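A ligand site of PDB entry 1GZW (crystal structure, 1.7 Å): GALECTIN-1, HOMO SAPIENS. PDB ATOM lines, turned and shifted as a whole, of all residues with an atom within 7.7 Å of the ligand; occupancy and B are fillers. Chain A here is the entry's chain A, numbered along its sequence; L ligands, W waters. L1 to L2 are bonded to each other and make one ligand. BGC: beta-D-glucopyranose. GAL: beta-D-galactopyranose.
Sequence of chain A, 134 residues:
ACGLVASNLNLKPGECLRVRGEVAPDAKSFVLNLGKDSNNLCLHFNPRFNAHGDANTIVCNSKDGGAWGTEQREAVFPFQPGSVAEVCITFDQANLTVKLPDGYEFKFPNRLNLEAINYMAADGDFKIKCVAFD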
ATOM      1  N   SER A  29      16.367  -0.083  14.589  1.00  0.00           N
ATOM      2  CA  SER A  29      15.000  -0.585  14.684  1.00  0.00           C
ATOM      3  C   SER A  29      14.046   0.596  14.564  1.00  0.00           C
ATOM      4  O   SER A  29      14.478   1.745  14.584  1.00  0.00           O
ATOM      5  CB  SER A  29      14.768  -1.246  16.043  1.00  0.00           C
ATOM      6  OG  SER A  29      14.649  -0.274  17.060  1.00  0.00           O
ATOM      7  N   PHE A  30      12.752   0.318  14.428  1.00  0.00           N
ATOM      8  CA  PHE A  30      11.755   1.374  14.373  1.00  0.00           C
ATOM      9  C   PHE A  30      10.518   0.918  15.125  1.00  0.00           C
ATOM     10  O   PHE A  30      10.344  -0.280  15.382  1.00  0.00           O
ATOM     11  CB  PHE A  30      11.446   1.790  12.920  1.00  0.00           C
ATOM     12  CG  PHE A  30      10.673   0.769  12.124  1.00  0.00           C
ATOM     13  CD1 PHE A  30       9.280   0.833  12.059  1.00  0.00           C
ATOM     14  CD2 PHE A  30      11.332  -0.202  11.390  1.00  0.00           C
ATOM     15  CE1 PHE A  30       8.564  -0.044  11.253  1.00  0.00           C
ATOM     16  CE2 PHE A  30      10.622  -1.099  10.579  1.00  0.00           C
ATOM     17  CZ  PHE A  30       9.238  -1.013  10.510  1.00  0.00           C
ATOM     18  N   VAL A  31       9.675   1.871  15.508  1.00  0.00           N
ATOM     19  CA  VAL A  31       8.486   1.561  16.291  1.00  0.00           C
ATOM     20  C   VAL A  31       7.202   2.220  15.801  1.00  0.00           C
ATOM     21  O   VAL A  31       7.207   3.348  15.318  1.00  0.00           O
ATOM     22  CB  VAL A  31       8.683   1.976  17.770  1.00  0.00           C
ATOM     23  CG1 VAL A  31       7.398   1.731  18.562  1.00  0.00           C
ATOM     24  CG2 VAL A  31       9.842   1.222  18.388  1.00  0.00           C
ATOM     25  N   ASN A  33       3.466   2.520  17.591  1.00  0.00           N
ATOM     26  CA  ASN A  33       2.659   2.246  18.777  1.00  0.00           C
ATOM     27  C   ASN A  33       1.191   2.567  18.557  1.00  0.00           C
ATOM     28  O   ASN A  33       0.847   3.558  17.917  1.00  0.00           O
ATOM     29  CB  ASN A  33       3.166   3.048  19.985  1.00  0.00           C
ATOM     30  CG  ASN A  33       4.515   2.585  20.476  1.00  0.00           C
ATOM     31  OD1 ASN A  33       4.794   1.390  20.524  1.00  0.00           O
ATOM     32  ND2 ASN A  33       5.361   3.538  20.874  1.00  0.00           N
ATOM     33  N   HIS A  44       2.666  -2.515  20.563  1.00  0.00           N
ATOM     34  CA  HIS A  44       3.965  -1.883  20.419  1.00  0.00           C
ATOM     35  C   HIS A  44       4.601  -2.754  19.327  1.00  0.00           C
ATOM     36  O   HIS A  44       5.028  -3.875  19.597  1.00  0.00           O
ATOM     37  CB  HIS A  44       4.777  -1.982  21.719  1.00  0.00           C
ATOM     38  CG  HIS A  44       6.219  -1.623  21.573  1.00  0.00           C
ATOM     39  ND1 HIS A  44       6.647  -0.329  21.316  1.00  0.00           N
ATOM     40  CD2 HIS A  44       7.350  -2.363  21.672  1.00  0.00           C
ATOM     41  CE1 HIS A  44       7.962  -0.306  21.256  1.00  0.00           C
ATOM     42  NE2 HIS A  44       8.413  -1.520  21.467  1.00  0.00           N
ATOM     43  N   PHE A  45       4.597  -2.255  18.095  1.00  0.00           N
ATOM     44  CA  PHE A  45       5.134  -2.953  16.931  1.00  0.00           C
ATOM     45  C   PHE A  45       6.582  -2.495  16.757  1.00  0.00           C
ATOM     46  O   PHE A  45       6.828  -1.371  16.314  1.00  0.00           O
ATOM     47  CB  PHE A  45       4.314  -2.607  15.691  1.00  0.00           C
ATOM     48  CG  PHE A  45       4.707  -3.354  14.447  1.00  0.00           C
ATOM     49  CD1 PHE A  45       4.412  -4.705  14.320  1.00  0.00           C
ATOM     50  CD2 PHE A  45       5.365  -2.697  13.418  1.00  0.00           C
ATOM     51  CE1 PHE A  45       4.775  -5.400  13.164  1.00  0.00           C
ATOM     52  CE2 PHE A  45       5.736  -3.390  12.266  1.00  0.00           C
ATOM     53  CZ  PHE A  45       5.441  -4.741  12.139  1.00  0.00           C
ATOM     54  N   ASN A  46       7.527  -3.375  17.079  1.00  0.00           N
ATOM     55  CA  ASN A  46       8.939  -3.012  17.060  1.00  0.00           C
ATOM     56  C   ASN A  46       9.904  -3.885  16.241  1.00  0.00           C
ATOM     57  O   ASN A  46      10.565  -4.770  16.794  1.00  0.00           O
ATOM     58  CB  ASN A  46       9.406  -2.965  18.522  1.00  0.00           C
ATOM     59  CG  ASN A  46      10.840  -2.484  18.688  1.00  0.00           C
ATOM     60  OD1 ASN A  46      11.443  -2.727  19.734  1.00  0.00           O
ATOM     61  ND2 ASN A  46      11.370  -1.809  17.682  1.00  0.00           N
ATOM     62  N   ARG A  48      13.133  -5.001  14.938  1.00  0.00           N
ATOM     63  CA  ARG A  48      14.506  -4.720  15.350  1.00  0.00           C
ATOM     64  C   ARG A  48      15.539  -5.286  14.368  1.00  0.00           C
ATOM     65  O   ARG A  48      15.601  -6.490  14.150  1.00  0.00           O
ATOM     66  CB  ARG A  48      14.778  -5.304  16.736  1.00  0.00           C
ATOM     67  CG  ARG A  48      13.920  -4.696  17.829  1.00  0.00           C
ATOM     68  CD  ARG A  48      14.159  -5.366  19.175  1.00  0.00           C
ATOM     69  NE  ARG A  48      13.291  -4.806  20.215  1.00  0.00           N
ATOM     70  CZ  ARG A  48      13.215  -5.260  21.454  1.00  0.00           C
ATOM     71  NH1 ARG A  48      13.955  -6.303  21.840  1.00  0.00           N
ATOM     72  NH2 ARG A  48      12.405  -4.682  22.325  1.00  0.00           N
ATOM     73  N   ALA A  51      19.089  -4.768  17.788  1.00  0.00           N
ATOM     74  CA  ALA A  51      18.877  -4.134  19.074  1.00  0.00           C
ATOM     75  C   ALA A  51      18.435  -5.106  20.153  1.00  0.00           C
ATOM     76  O   ALA A  51      17.689  -6.055  19.892  1.00  0.00           O
ATOM     77  CB  ALA A  51      17.842  -3.017  18.937  1.00  0.00           C
ATOM     78  N   HIS A  52      18.907  -4.868  21.373  1.00  0.00           N
ATOM     79  CA  HIS A  52      18.560  -5.698  22.525  1.00  0.00           C
ATOM     80  C   HIS A  52      18.769  -7.187  22.323  1.00  0.00           C
ATOM     81  O   HIS A  52      17.996  -8.000  22.822  1.00  0.00           O
ATOM     82  CB  HIS A  52      17.111  -5.430  22.929  1.00  0.00           C
ATOM     83  CG  HIS A  52      16.810  -3.983  23.148  1.00  0.00           C
ATOM     84  ND1 HIS A  52      17.328  -3.269  24.211  1.00  0.00           N
ATOM     85  CD2 HIS A  52      16.058  -3.108  22.440  1.00  0.00           C
ATOM     86  CE1 HIS A  52      16.915  -2.018  24.137  1.00  0.00           C
ATOM     87  NE2 HIS A  52      16.150  -1.887  23.073  1.00  0.00           N
ATOM     88  N   GLY A  53      19.813  -7.547  21.584  1.00  0.00           N
ATOM     89  CA  GLY A  53      20.083  -8.951  21.342  1.00  0.00           C
ATOM     90  C   GLY A  53      19.328  -9.537  20.162  1.00  0.00           C
ATOM     91  O   GLY A  53      19.591 -10.666  19.760  1.00  0.00           O
ATOM     92  N   ASP A  54      18.391  -8.765  19.615  1.00  0.00           N
ATOM     93  CA  ASP A  54      17.620  -9.229  18.468  1.00  0.00           C
ATOM     94  C   ASP A  54      18.244  -8.821  17.144  1.00  0.00           C
ATOM     95  O   ASP A  54      18.736  -7.697  16.981  1.00  0.00           O
ATOM     96  CB  ASP A  54      16.184  -8.683  18.533  1.00  0.00           C
ATOM     97  CG  ASP A  54      15.380  -9.290  19.656  1.00  0.00           C
ATOM     98  OD1 ASP A  54      14.951  -8.538  20.558  1.00  0.00           O
ATOM     99  OD2 ASP A  54      15.181 -10.518  19.656  1.00  0.00           O
ATOM    100  N   VAL A  59       9.449  -7.606  17.195  1.00  0.00           N
ATOM    101  CA  VAL A  59       9.073  -7.785  18.594  1.00  0.00           C
ATOM    102  C   VAL A  59       7.807  -6.985  18.839  1.00  0.00           C
ATOM    103  O   VAL A  59       7.730  -5.810  18.481  1.00  0.00           O
ATOM    104  CB  VAL A  59      10.172  -7.256  19.557  1.00  0.00           C
ATOM    105  CG1 VAL A  59       9.699  -7.382  20.995  1.00  0.00           C
ATOM    106  CG2 VAL A  59      11.461  -8.029  19.348  1.00  0.00           C
ATOM    107  N   CYS A  60       6.797  -7.633  19.434  1.00  0.00           N
ATOM    108  CA  CYS A  60       5.540  -6.962  19.753  1.00  0.00           C
ATOM    109  C   CYS A  60       5.269  -7.076  21.236  1.00  0.00           C
ATOM    110  O   CYS A  60       5.637  -8.064  21.872  1.00  0.00           O
ATOM    111  CB  CYS A  60       4.377  -7.588  18.979  1.00  0.00           C
ATOM    112  SG  CYS A  60       4.373  -7.222  17.204  1.00  0.00           S
ATOM    113  N   ASN A  61       4.622  -6.066  21.795  1.00  0.00           N
ATOM    114  CA  ASN A  61       4.304  -6.106  23.207  1.00  0.00           C
ATOM    115  C   ASN A  61       3.171  -5.160  23.494  1.00  0.00           C
ATOM    116  O   ASN A  61       2.763  -4.374  22.625  1.00  0.00           O
ATOM    117  CB  ASN A  61       5.539  -5.715  24.040  1.00  0.00           C
ATOM    118  CG  ASN A  61       5.499  -6.264  25.470  1.00  0.00           C
ATOM    119  OD1 ASN A  61       6.456  -6.122  26.227  1.00  0.00           O
ATOM    120  ND2 ASN A  61       4.384  -6.881  25.831  1.00  0.00           N
ATOM    121  N   SER A  62       2.627  -5.264  24.700  1.00  0.00           N
ATOM    122  CA  SER A  62       1.547  -4.400  25.139  1.00  0.00           C
ATOM    123  C   SER A  62       2.164  -3.567  26.251  1.00  0.00           C
ATOM    124  O   SER A  62       3.249  -3.883  26.739  1.00  0.00           O
ATOM    125  CB  SER A  62       0.401  -5.237  25.690  1.00  0.00           C
ATOM    126  OG  SER A  62       0.849  -6.068  26.745  1.00  0.00           O
ATOM    127  N   LYS A  63       1.485  -2.489  26.621  1.00  0.00           N
ATOM    128  CA  LYS A  63       1.970  -1.628  27.692  1.00  0.00           C
ATOM    129  C   LYS A  63       0.733  -1.249  28.494  1.00  0.00           C
ATOM    130  O   LYS A  63      -0.216  -0.679  27.956  1.00  0.00           O
ATOM    131  CB  LYS A  63       2.647  -0.376  27.131  1.00  0.00           C
ATOM    132  CG  LYS A  63       3.534   0.340  28.132  1.00  0.00           C
ATOM    133  CD  LYS A  63       4.422   1.357  27.438  1.00  0.00           C
ATOM    134  CE  LYS A  63       5.556   1.822  28.332  1.00  0.00           C
ATOM    135  NZ  LYS A  63       6.473   2.733  27.597  1.00  0.00           N
ATOM    136  N   TRP A  68       5.531  -2.746  30.568  1.00  0.00           N
ATOM    137  CA  TRP A  68       5.617  -3.627  29.401  1.00  0.00           C
ATOM    138  C   TRP A  68       5.076  -5.011  29.737  1.00  0.00           C
ATOM    139  O   TRP A  68       5.324  -5.533  30.828  1.00  0.00           O
ATOM    140  CB  TRP A  68       7.068  -3.762  28.943  1.00  0.00           C
ATOM    141  CG  TRP A  68       7.636  -2.546  28.296  1.00  0.00           C
ATOM    142  CD1 TRP A  68       8.712  -1.823  28.705  1.00  0.00           C
ATOM    143  CD2 TRP A  68       7.163  -1.923  27.095  1.00  0.00           C
ATOM    144  NE1 TRP A  68       8.946  -0.782  27.838  1.00  0.00           N
ATOM    145  CE2 TRP A  68       8.011  -0.823  26.839  1.00  0.00           C
ATOM    146  CE3 TRP A  68       6.107  -2.182  26.217  1.00  0.00           C
ATOM    147  CZ2 TRP A  68       7.837   0.017  25.730  1.00  0.00           C
ATOM    148  CZ3 TRP A  68       5.933  -1.341  25.108  1.00  0.00           C
ATOM    149  CH2 TRP A  68       6.793  -0.259  24.882  1.00  0.00           C
ATOM    150  N   GLY A  69       4.353  -5.604  28.794  1.00  0.00           N
ATOM    151  CA  GLY A  69       3.808  -6.927  29.001  1.00  0.00           C
ATOM    152  C   GLY A  69       4.806  -7.970  28.545  1.00  0.00           C
ATOM    153  O   GLY A  69       6.007  -7.693  28.461  1.00  0.00           O
ATOM    154  N   THR A  70       4.329  -9.175  28.250  1.00  0.00           N
ATOM    155  CA  THR A  70       5.190 -10.253  27.788  1.00  0.00           C
ATOM    156  C   THR A  70       5.377 -10.111  26.280  1.00  0.00           C
ATOM    157  O   THR A  70       4.407 -10.061  25.525  1.00  0.00           O
ATOM    158  CB  THR A  70       4.559 -11.625  28.095  1.00  0.00           C
ATOM    159  OG1 THR A  70       4.308 -11.726  29.509  1.00  0.00           O
ATOM    160  CG2 THR A  70       5.494 -12.754  27.662  1.00  0.00           C
ATOM    161  N   GLU A  71       6.632 -10.038  25.844  1.00  0.00           N
ATOM    162  CA  GLU A  71       6.931  -9.872  24.422  1.00  0.00           C
ATOM    163  C   GLU A  71       6.588 -11.083  23.562  1.00  0.00           C
ATOM    164  O   GLU A  71       6.615 -12.221  24.030  1.00  0.00           O
ATOM    165  CB  GLU A  71       8.419  -9.553  24.220  1.00  0.00           C
ATOM    166  CG  GLU A  71       8.906  -8.315  24.962  1.00  0.00           C
ATOM    167  CD  GLU A  71      10.393  -8.086  24.798  1.00  0.00           C
ATOM    168  OE1 GLU A  71      11.132  -9.076  24.640  1.00  0.00           O
ATOM    169  OE2 GLU A  71      10.822  -6.907  24.833  1.00  0.00           O
ATOM    170  N   GLN A  72       6.275 -10.805  22.305  1.00  0.00           N
ATOM    171  CA  GLN A  72       5.970 -11.832  21.322  1.00  0.00           C
ATOM    172  C   GLN A  72       6.908 -11.559  20.146  1.00  0.00           C
ATOM    173  O   GLN A  72       7.168 -10.396  19.821  1.00  0.00           O
ATOM    174  CB  GLN A  72       4.506 -11.736  20.860  1.00  0.00           C
ATOM    175  CG  GLN A  72       4.127 -12.752  19.793  1.00  0.00           C
ATOM    176  CD  GLN A  72       2.644 -12.742  19.471  1.00  0.00           C
ATOM    177  OE1 GLN A  72       1.807 -13.088  20.310  1.00  0.00           O
ATOM    178  NE2 GLN A  72       2.307 -12.344  18.240  1.00  0.00           N
ATOM    179  N   ARG A  73       7.442 -12.605  19.531  1.00  0.00           N
ATOM    180  CA  ARG A  73       8.354 -12.447  18.405  1.00  0.00           C
ATOM    181  C   ARG A  73       7.866 -13.238  17.199  1.00  0.00           C
ATOM    182  O   ARG A  73       7.311 -14.329  17.363  1.00  0.00           O
ATOM    183  CB  ARG A  73       9.771 -12.890  18.820  1.00  0.00           C
ATOM    184  CG  ARG A  73      10.476 -11.879  19.732  1.00  0.00           C
ATOM    185  CD  ARG A  73      11.843 -12.378  20.177  1.00  0.00           C
ATOM    186  NE  ARG A  73      12.634 -11.297  20.776  1.00  0.00           N
ATOM    187  CZ  ARG A  73      12.340 -10.694  21.919  1.00  0.00           C
ATOM    188  NH1 ARG A  73      11.277 -11.069  22.631  1.00  0.00           N
ATOM    189  NH2 ARG A  73      13.096  -9.693  22.367  1.00  0.00           N
HETATM  190  C2  BGC L   1      14.211  -7.560  26.553  1.00  0.00           C
HETATM  191  C3  BGC L   1      14.267  -6.310  25.670  1.00  0.00           C
HETATM  192  C4  BGC L   1      13.763  -5.122  26.513  1.00  0.00           C
HETATM  193  C5  BGC L   1      14.634  -4.962  27.803  1.00  0.00           C
HETATM  194  C6  BGC L   1      14.177  -3.831  28.733  1.00  0.00           C
HETATM  195  C1  BGC L   1      15.075  -7.353  27.817  1.00  0.00           C
HETATM  196  O1  BGC L   1      14.990  -8.484  28.623  1.00  0.00           O
HETATM  197  O2  BGC L   1      14.688  -8.695  25.815  1.00  0.00           O
HETATM  198  O3  BGC L   1      13.351  -6.527  24.585  1.00  0.00           O
HETATM  199  O4  BGC L   1      13.797  -3.912  25.713  1.00  0.00           O
HETATM  200  O5  BGC L   1      14.608  -6.201  28.576  1.00  0.00           O
HETATM  201  O6  BGC L   1      12.828  -4.026  29.178  1.00  0.00           O
HETATM  202  C1  GAL L   2      12.659  -3.086  25.643  1.00  0.00           C
HETATM  203  C2  GAL L   2      12.991  -1.883  24.722  1.00  0.00           C
HETATM  204  C3  GAL L   2      11.747  -0.979  24.654  1.00  0.00           C
HETATM  205  C4  GAL L   2      10.584  -1.781  24.038  1.00  0.00           C
HETATM  206  C5  GAL L   2      10.318  -2.995  24.967  1.00  0.00           C
HETATM  207  C6  GAL L   2       9.213  -3.883  24.426  1.00  0.00           C
HETATM  208  O2  GAL L   2      14.091  -1.166  25.292  1.00  0.00           O
HETATM  209  O3  GAL L   2      12.036   0.137  23.807  1.00  0.00           O
HETATM  210  O4  GAL L   2      10.936  -2.215  22.735  1.00  0.00           O
HETATM  211  O5  GAL L   2      11.533  -3.813  25.084  1.00  0.00           O
HETATM  212  O6  GAL L   2       9.017  -4.973  25.327  1.00  0.00           O
HETATM  213  O   HOH W   1      10.274   2.407  23.401  1.00  0.00           O
HETATM  214  O   HOH W   2      12.975 -10.774  25.947  1.00  0.00           O
HETATM  215  O   HOH W   3      12.472  -0.406  20.913  1.00  0.00           O
HETATM  216  O   HOH W   4      10.115  -5.248  27.967  1.00  0.00           O
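Merely in contact with the ligand: Trp 68 and Arg 73. Hydrophobic or aromatic side chains that line the ligand: His 44, His 52 and Trp 68. Of the 23 residues printed, 8 come within 4 Å of the ligand. The nearest printed residue that does not touch the ligand is Asp 54 (4.8 Å).
Water W2 bridges O2 of BGC L1 (2.7 Å) and OE1 of Glu 71 (2.8 Å). Water W3 bridges the side-chain amide oxygen of Asn 46 and an oxygen (O3) of GAL L2.
The side-chain carboxylate (OE2) of Glu 71 is in salt-bridge range of the guanidinium group (NH2) of Arg 48 (3.7 Å). ND2 of Asn 46 sits at hydrogen-bond distance from O of Phe 30 (2.9 Å). The guanidinium group (NE) of Arg 48 lies within hydrogen-bond range of the side-chain amide oxygen (OD1) of Asn 46. The side-chain amide nitrogen of Asn 61 is in hydrogen-bond range of the backbone carbonyl oxygen of Thr 70 (3.2 Å). The backbone NH (N) of Asn 46 lies within hydrogen-bond range of the backbone carbonyl oxygen (O) of Val 59 (2.8 Å). The backbone NH (N) of His 44 sits at hydrogen-bond distance from the backbone carbonyl oxygen (O) of Asn 61, 2.8 Å away. The side-chain carboxylate (OE1) of Glu 71 lies within salt-bridge range of the guanidinium group (NH1) of Arg 73, 2.8 Å away. NH2 of Arg 73 lies within salt-bridge range of OD1 of Asp 54.
An oxygen (O4) of GAL L2 sits at hydrogen-bond distance from a ring nitrogen (NE2) of His 44 (2.9 Å). O4 of GAL L2 sits at hydrogen-bond distance from OD1 of Asn 46, 3.1 Å away. The guanidinium group of Arg 48 is in hydrogen-bond range of an oxygen (O3) of BGC L1. The side-chain carboxylate of Glu 71 is in hydrogen-bond range of an oxygen (O3) of BGC L1 (2.6 Å). O2 of GAL L2 lies within hydrogen-bond range of NE2 of His 52, 3.1 Å away. The side-chain amide oxygen of Asn 61 is in hydrogen-bond range of an oxygen (O6) of GAL L2 (2.9 Å).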
